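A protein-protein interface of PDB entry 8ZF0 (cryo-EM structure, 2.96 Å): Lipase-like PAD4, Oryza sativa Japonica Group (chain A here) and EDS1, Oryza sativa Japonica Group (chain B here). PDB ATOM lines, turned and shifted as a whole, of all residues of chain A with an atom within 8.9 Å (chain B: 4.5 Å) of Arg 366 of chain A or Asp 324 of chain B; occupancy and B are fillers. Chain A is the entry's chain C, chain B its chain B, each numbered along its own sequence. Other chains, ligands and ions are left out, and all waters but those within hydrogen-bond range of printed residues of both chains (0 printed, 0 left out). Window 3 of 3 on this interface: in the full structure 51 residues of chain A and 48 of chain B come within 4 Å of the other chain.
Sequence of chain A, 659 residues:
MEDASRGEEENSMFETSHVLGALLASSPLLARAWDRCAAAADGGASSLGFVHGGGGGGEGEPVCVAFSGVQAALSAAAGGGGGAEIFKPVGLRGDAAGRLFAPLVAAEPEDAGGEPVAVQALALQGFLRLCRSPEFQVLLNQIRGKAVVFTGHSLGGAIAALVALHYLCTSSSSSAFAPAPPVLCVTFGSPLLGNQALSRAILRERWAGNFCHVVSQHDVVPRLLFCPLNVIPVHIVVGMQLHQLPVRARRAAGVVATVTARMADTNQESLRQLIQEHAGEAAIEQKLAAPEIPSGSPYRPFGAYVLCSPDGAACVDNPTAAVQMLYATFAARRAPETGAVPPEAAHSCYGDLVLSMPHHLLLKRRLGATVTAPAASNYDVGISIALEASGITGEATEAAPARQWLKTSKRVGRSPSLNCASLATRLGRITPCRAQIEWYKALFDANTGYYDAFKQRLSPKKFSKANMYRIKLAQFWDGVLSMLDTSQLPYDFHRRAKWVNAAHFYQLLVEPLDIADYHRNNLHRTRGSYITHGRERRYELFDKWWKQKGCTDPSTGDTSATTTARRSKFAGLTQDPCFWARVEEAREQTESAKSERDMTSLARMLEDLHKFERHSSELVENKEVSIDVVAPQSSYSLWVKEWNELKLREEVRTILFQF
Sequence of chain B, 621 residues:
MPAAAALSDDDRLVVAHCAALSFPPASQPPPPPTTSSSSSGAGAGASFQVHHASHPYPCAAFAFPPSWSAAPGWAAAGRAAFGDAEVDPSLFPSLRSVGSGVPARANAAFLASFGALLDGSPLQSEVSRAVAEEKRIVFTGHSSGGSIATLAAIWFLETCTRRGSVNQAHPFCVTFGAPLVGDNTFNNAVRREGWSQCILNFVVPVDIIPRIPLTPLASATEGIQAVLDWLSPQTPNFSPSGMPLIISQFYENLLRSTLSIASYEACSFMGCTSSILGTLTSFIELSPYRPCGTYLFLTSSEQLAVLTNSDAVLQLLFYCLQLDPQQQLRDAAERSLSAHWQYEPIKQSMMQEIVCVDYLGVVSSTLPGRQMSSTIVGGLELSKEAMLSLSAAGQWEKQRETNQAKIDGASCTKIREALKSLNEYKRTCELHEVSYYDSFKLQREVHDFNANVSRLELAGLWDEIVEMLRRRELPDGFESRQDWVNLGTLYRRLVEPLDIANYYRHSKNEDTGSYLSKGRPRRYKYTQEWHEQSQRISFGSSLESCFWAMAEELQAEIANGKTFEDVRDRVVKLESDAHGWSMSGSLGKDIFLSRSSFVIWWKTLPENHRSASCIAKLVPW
The backbone NH of Leu 323 of chain B sits at hydrogen-bond distance from the backbone carbonyl oxygen of Leu 362 of chain A (3.1 Å). The backbone carbonyl oxygen (O) of Leu 323 of chain B is in hydrogen-bond range of the backbone NH (N) of Lys 364 of chain A. NH2 of Arg 366 of chain A is in salt-bridge range of OD2 of Asp 324 of chain B (3.4 Å). The side-chain carboxylate (OE2) of Glu 381 of chain B lies within salt-bridge range of the side-chain amino group (NZ) of Lys 364 of chain A, 3.7 Å away. The side-chain carboxylate (OE2) of Glu 381 of chain B lies within salt-bridge range of the guanidinium group (NH1) of Arg 366 of chain A (2.6 Å). NZ of Lys 384 of chain B sits at hydrogen-bond distance from O of Arg 365 of chain A (2.9 Å). The side-chain amino group of Lys 384 of chain B sits close to the backbone NH of Leu 367 of chain A.
The side-chain amide oxygen (OE1) of Gln 327 of chain B lies close to the side-chain carboxylate (OD1) of Asp 324 of chain B, 2.9 Å away. O of Lys 364 of chain A is in hydrogen-bond range of NE of Arg 366 of chain A.
CD2 of Leu 363 of chain A touches CD2 of Leu 323 of chain B (3.7 Å). CB of Gln 322 of chain B touches CB of Lys 364 of chain A, 3.6 Å away. Lys 364 of chain A touches Pro 325 of chain B. Pro 325 of chain B touches Arg 366 of chain A (CD to NH2, 3.5 Å). C of Arg 366 of chain A touches NZ of Lys 384 of chain B, at 3.7 Å.
Of the printed residues of chain B, Leu 363 of chain A touches Leu 323 (3.7 Å). Of the printed residues of chain B, Lys 364 of chain A touches Gln 322, Leu 323, Pro 325 and Glu 381. Of the printed residues of chain B, Arg 365 of chain A touches Lys 384. Arg 366 of chain A touches just these residues of chain B: Asp 324 (3.4 Å), Pro 325 (3.5 Å), Glu 381 (2.6 Å) and Lys 384 (3.7 Å). Of the printed residues of chain B, Leu 367 of chain A touches Lys 384. Leu 323 of chain B touches just these residues of chain A: Leu 362 (3.1 Å), Leu 363 (3.7 Å) and Lys 364 (2.8 Å). Of chain A, only Lys 364 (3.8 Å) and Arg 366 (3.5 Å) come within 4 Å of Pro 325 of chain B. Gln 327 of chain B touches none of the printed residues of chain A. Of the printed residues of chain A, Glu 381 of chain B touches Lys 364 (3.7 Å) and Arg 366 (2.6 Å). The nearest residue of chain A that does not touch Asp 324 of chain B is Leu 363 of chain A (4.3 Å).
Hydrophobic or aromatic side chains of chain B within 4 Å of the printed part of chain A: Leu 323 and Pro 325. Along chain B the printed residues that touch a printed residue of chain A span positions 322 to 384. Of the 8 printed residues of chain A, 6 touch a printed residue of chain B. Hydrophobic or aromatic side chains of chain A within 4 Å of the printed part of chain B: Leu 363 and Leu 367. Along chain A the printed residues that touch a printed residue of chain B span positions 362 to 367. Among the printed residues, 12 pairs touch across the chains.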
ATOM      1  N   HIS A 359       1.331 -26.135   7.971  1.00  0.00           N
ATOM      2  CA  HIS A 359       2.750 -26.398   7.753  1.00  0.00           C
ATOM      3  C   HIS A 359       3.602 -25.784   8.857  1.00  0.00           C
ATOM      4  O   HIS A 359       4.542 -26.418   9.350  1.00  0.00           O
ATOM      5  CB  HIS A 359       3.176 -25.868   6.384  1.00  0.00           C
ATOM      6  CG  HIS A 359       4.652 -25.661   6.248  1.00  0.00           C
ATOM      7  ND1 HIS A 359       5.214 -24.420   6.040  1.00  0.00           N
ATOM      8  CD2 HIS A 359       5.682 -26.539   6.289  1.00  0.00           C
ATOM      9  CE1 HIS A 359       6.527 -24.541   5.960  1.00  0.00           C
ATOM     10  NE2 HIS A 359       6.837 -25.817   6.107  1.00  0.00           N
ATOM     11  N   LEU A 362       3.206 -27.705  12.085  1.00  0.00           N
ATOM     12  CA  LEU A 362       3.867 -29.003  12.078  1.00  0.00           C
ATOM     13  C   LEU A 362       5.384 -28.897  12.185  1.00  0.00           C
ATOM     14  O   LEU A 362       6.074 -29.914  12.048  1.00  0.00           O
ATOM     15  CB  LEU A 362       3.489 -29.781  10.815  1.00  0.00           C
ATOM     16  CG  LEU A 362       2.063 -30.333  10.760  1.00  0.00           C
ATOM     17  CD1 LEU A 362       1.891 -31.258   9.566  1.00  0.00           C
ATOM     18  CD2 LEU A 362       1.713 -31.051  12.054  1.00  0.00           C
ATOM     19  N   LEU A 363       5.918 -27.703  12.424  1.00  0.00           N
ATOM     20  CA  LEU A 363       7.357 -27.490  12.524  1.00  0.00           C
ATOM     21  C   LEU A 363       7.760 -27.322  13.983  1.00  0.00           C
ATOM     22  O   LEU A 363       7.119 -26.571  14.727  1.00  0.00           O
ATOM     23  CB  LEU A 363       7.787 -26.263  11.717  1.00  0.00           C
ATOM     24  CG  LEU A 363       7.666 -26.353  10.196  1.00  0.00           C
ATOM     25  CD1 LEU A 363       8.457 -25.237   9.530  1.00  0.00           C
ATOM     26  CD2 LEU A 363       8.129 -27.712   9.697  1.00  0.00           C
ATOM     27  N   LYS A 364       8.821 -28.023  14.386  1.00  0.00           N
ATOM     28  CA  LYS A 364       9.354 -27.928  15.746  1.00  0.00           C
ATOM     29  C   LYS A 364      10.397 -26.814  15.783  1.00  0.00           C
ATOM     30  O   LYS A 364      11.601 -27.035  15.639  1.00  0.00           O
ATOM     31  CB  LYS A 364       9.937 -29.263  16.188  1.00  0.00           C
ATOM     32  CG  LYS A 364      10.207 -29.361  17.681  1.00  0.00           C
ATOM     33  CD  LYS A 364      10.656 -30.760  18.073  1.00  0.00           C
ATOM     34  CE  LYS A 364      11.803 -31.241  17.198  1.00  0.00           C
ATOM     35  NZ  LYS A 364      12.274 -32.596  17.595  1.00  0.00           N
ATOM     36  N   ARG A 365       9.913 -25.591  15.981  1.00  0.00           N
ATOM     37  CA  ARG A 365      10.796 -24.434  16.042  1.00  0.00           C
ATOM     38  C   ARG A 365      11.466 -24.360  17.409  1.00  0.00           C
ATOM     39  O   ARG A 365      10.789 -24.261  18.438  1.00  0.00           O
ATOM     40  CB  ARG A 365      10.012 -23.155  15.753  1.00  0.00           C
ATOM     41  CG  ARG A 365       8.634 -23.107  16.395  1.00  0.00           C
ATOM     42  CD  ARG A 365       7.836 -21.911  15.903  1.00  0.00           C
ATOM     43  NE  ARG A 365       7.179 -22.179  14.629  1.00  0.00           N
ATOM     44  CZ  ARG A 365       7.372 -21.475  13.522  1.00  0.00           C
ATOM     45  NH1 ARG A 365       8.204 -20.447  13.494  1.00  0.00           N
ATOM     46  NH2 ARG A 365       6.714 -21.811  12.417  1.00  0.00           N
ATOM     47  N   ARG A 366      12.795 -24.418  17.421  1.00  0.00           N
ATOM     48  CA  ARG A 366      13.536 -24.340  18.671  1.00  0.00           C
ATOM     49  C   ARG A 366      13.481 -22.927  19.239  1.00  0.00           C
ATOM     50  O   ARG A 366      13.562 -21.940  18.502  1.00  0.00           O
ATOM     51  CB  ARG A 366      14.991 -24.760  18.454  1.00  0.00           C
ATOM     52  CG  ARG A 366      15.174 -25.903  17.468  1.00  0.00           C
ATOM     53  CD  ARG A 366      14.646 -27.213  18.026  1.00  0.00           C
ATOM     54  NE  ARG A 366      14.475 -28.220  16.986  1.00  0.00           N
ATOM     55  CZ  ARG A 366      15.197 -29.328  16.889  1.00  0.00           C
ATOM     56  NH1 ARG A 366      16.154 -29.607  17.758  1.00  0.00           N
ATOM     57  NH2 ARG A 366      14.952 -30.177  15.894  1.00  0.00           N
ATOM     58  N   LEU A 367      13.340 -22.834  20.559  1.00  0.00           N
ATOM     59  CA  LEU A 367      13.339 -21.537  21.222  1.00  0.00           C
ATOM     60  C   LEU A 367      14.727 -20.911  21.166  1.00  0.00           C
ATOM     61  O   LEU A 367      15.740 -21.604  21.308  1.00  0.00           O
ATOM     62  CB  LEU A 367      12.880 -21.681  22.672  1.00  0.00           C
ATOM     63  CG  LEU A 367      12.136 -20.480  23.265  1.00  0.00           C
ATOM     64  CD1 LEU A 367      10.711 -20.400  22.741  1.00  0.00           C
ATOM     65  CD2 LEU A 367      12.147 -20.544  24.785  1.00  0.00           C
ATOM     66  N   GLY A 368      14.772 -19.600  20.957  1.00  0.00           N
ATOM     67  CA  GLY A 368      16.029 -18.880  20.888  1.00  0.00           C
ATOM     68  C   GLY A 368      15.959 -17.496  21.502  1.00  0.00           C
ATOM     69  O   GLY A 368      14.920 -17.090  22.023  1.00  0.00           O
ATOM     70  N   GLN B 322       7.266 -34.065  15.492  1.00  0.00           N
ATOM     71  CA  GLN B 322       7.285 -32.752  14.863  1.00  0.00           C
ATOM     72  C   GLN B 322       8.499 -32.612  13.954  1.00  0.00           C
ATOM     73  O   GLN B 322       9.596 -33.077  14.276  1.00  0.00           O
ATOM     74  CB  GLN B 322       7.285 -31.654  15.926  1.00  0.00           C
ATOM     75  CG  GLN B 322       5.979 -31.538  16.696  1.00  0.00           C
ATOM     76  CD  GLN B 322       5.856 -30.227  17.444  1.00  0.00           C
ATOM     77  OE1 GLN B 322       6.677 -29.911  18.305  1.00  0.00           O
ATOM     78  NE2 GLN B 322       4.827 -29.454  17.118  1.00  0.00           N
ATOM     79  N   LEU B 323       8.293 -31.970  12.808  1.00  0.00           N
ATOM     80  CA  LEU B 323       9.337 -31.871  11.799  1.00  0.00           C
ATOM     81  C   LEU B 323      10.476 -30.972  12.268  1.00  0.00           C
ATOM     82  O   LEU B 323      10.273 -29.995  12.994  1.00  0.00           O
ATOM     83  CB  LEU B 323       8.756 -31.339  10.488  1.00  0.00           C
ATOM     84  CG  LEU B 323       9.638 -31.463   9.244  1.00  0.00           C
ATOM     85  CD1 LEU B 323      10.060 -32.908   9.033  1.00  0.00           C
ATOM     86  CD2 LEU B 323       8.915 -30.931   8.018  1.00  0.00           C
ATOM     87  N   ASP B 324      11.688 -31.318  11.842  1.00  0.00           N
ATOM     88  CA  ASP B 324      12.863 -30.527  12.158  1.00  0.00           C
ATOM     89  C   ASP B 324      12.828 -29.202  11.395  1.00  0.00           C
ATOM     90  O   ASP B 324      12.134 -29.076  10.384  1.00  0.00           O
ATOM     91  CB  ASP B 324      14.130 -31.307  11.815  1.00  0.00           C
ATOM     92  CG  ASP B 324      14.374 -32.465  12.763  1.00  0.00           C
ATOM     93  OD1 ASP B 324      13.524 -33.378  12.821  1.00  0.00           O
ATOM     94  OD2 ASP B 324      15.416 -32.463  13.450  1.00  0.00           O
ATOM     95  N   PRO B 325      13.559 -28.189  11.878  1.00  0.00           N
ATOM     96  CA  PRO B 325      13.544 -26.888  11.182  1.00  0.00           C
ATOM     97  C   PRO B 325      13.971 -26.967   9.727  1.00  0.00           C
ATOM     98  O   PRO B 325      13.427 -26.239   8.889  1.00  0.00           O
ATOM     99  CB  PRO B 325      14.514 -26.033  12.015  1.00  0.00           C
ATOM    100  CG  PRO B 325      15.253 -26.998  12.899  1.00  0.00           C
ATOM    101  CD  PRO B 325      14.311 -28.125  13.141  1.00  0.00           C
ATOM    102  N   GLN B 326      14.932 -27.831   9.397  1.00  0.00           N
ATOM    103  CA  GLN B 326      15.403 -28.006   8.023  1.00  0.00           C
ATOM    104  C   GLN B 326      15.312 -29.490   7.679  1.00  0.00           C
ATOM    105  O   GLN B 326      16.290 -30.231   7.819  1.00  0.00           O
ATOM    106  CB  GLN B 326      16.822 -27.473   7.853  1.00  0.00           C
ATOM    107  CG  GLN B 326      16.957 -25.978   8.091  1.00  0.00           C
ATOM    108  CD  GLN B 326      18.355 -25.467   7.804  1.00  0.00           C
ATOM    109  OE1 GLN B 326      19.240 -26.230   7.419  1.00  0.00           O
ATOM    110  NE2 GLN B 326      18.560 -24.169   7.992  1.00  0.00           N
ATOM    111  N   GLN B 327      14.136 -29.917   7.224  1.00  0.00           N
ATOM    112  CA  GLN B 327      13.918 -31.299   6.823  1.00  0.00           C
ATOM    113  C   GLN B 327      12.645 -31.370   5.995  1.00  0.00           C
ATOM    114  O   GLN B 327      11.701 -30.608   6.217  1.00  0.00           O
ATOM    115  CB  GLN B 327      13.822 -32.231   8.038  1.00  0.00           C
ATOM    116  CG  GLN B 327      13.912 -33.711   7.699  1.00  0.00           C
ATOM    117  CD  GLN B 327      13.837 -34.597   8.926  1.00  0.00           C
ATOM    118  OE1 GLN B 327      13.692 -34.111  10.048  1.00  0.00           O
ATOM    119  NE2 GLN B 327      13.935 -35.905   8.719  1.00  0.00           N
ATOM    120  N   GLU B 381      14.056 -33.949  23.083  1.00  0.00           N
ATOM    121  CA  GLU B 381      13.970 -32.492  22.992  1.00  0.00           C
ATOM    122  C   GLU B 381      12.564 -32.117  22.537  1.00  0.00           C
ATOM    123  O   GLU B 381      12.286 -31.968  21.346  1.00  0.00           O
ATOM    124  CB  GLU B 381      15.032 -31.947  22.046  1.00  0.00           C
ATOM    125  CG  GLU B 381      15.329 -32.844  20.854  1.00  0.00           C
ATOM    126  CD  GLU B 381      16.214 -32.170  19.825  1.00  0.00           C
ATOM    127  OE1 GLU B 381      17.351 -31.789  20.176  1.00  0.00           O
ATOM    128  OE2 GLU B 381      15.774 -32.020  18.666  1.00  0.00           O
ATOM    129  N   LYS B 384       7.879 -26.295  23.236  1.00  0.00           N
ATOM    130  CA  LYS B 384       7.300 -25.480  24.301  1.00  0.00           C
ATOM    131  C   LYS B 384       5.853 -25.870  24.571  1.00  0.00           C
ATOM    132  O   LYS B 384       5.430 -25.940  25.731  1.00  0.00           O
ATOM    133  CB  LYS B 384       7.401 -23.996  23.943  1.00  0.00           C
ATOM    134  CG  LYS B 384       8.721 -23.329  24.324  1.00  0.00           C
ATOM    135  CD  LYS B 384       9.910 -23.926  23.583  1.00  0.00           C
ATOM    136  CE  LYS B 384       9.741 -23.813  22.076  1.00  0.00           C
ATOM    137  NZ  LYS B 384      10.844 -24.492  21.342  1.00  0.00           N
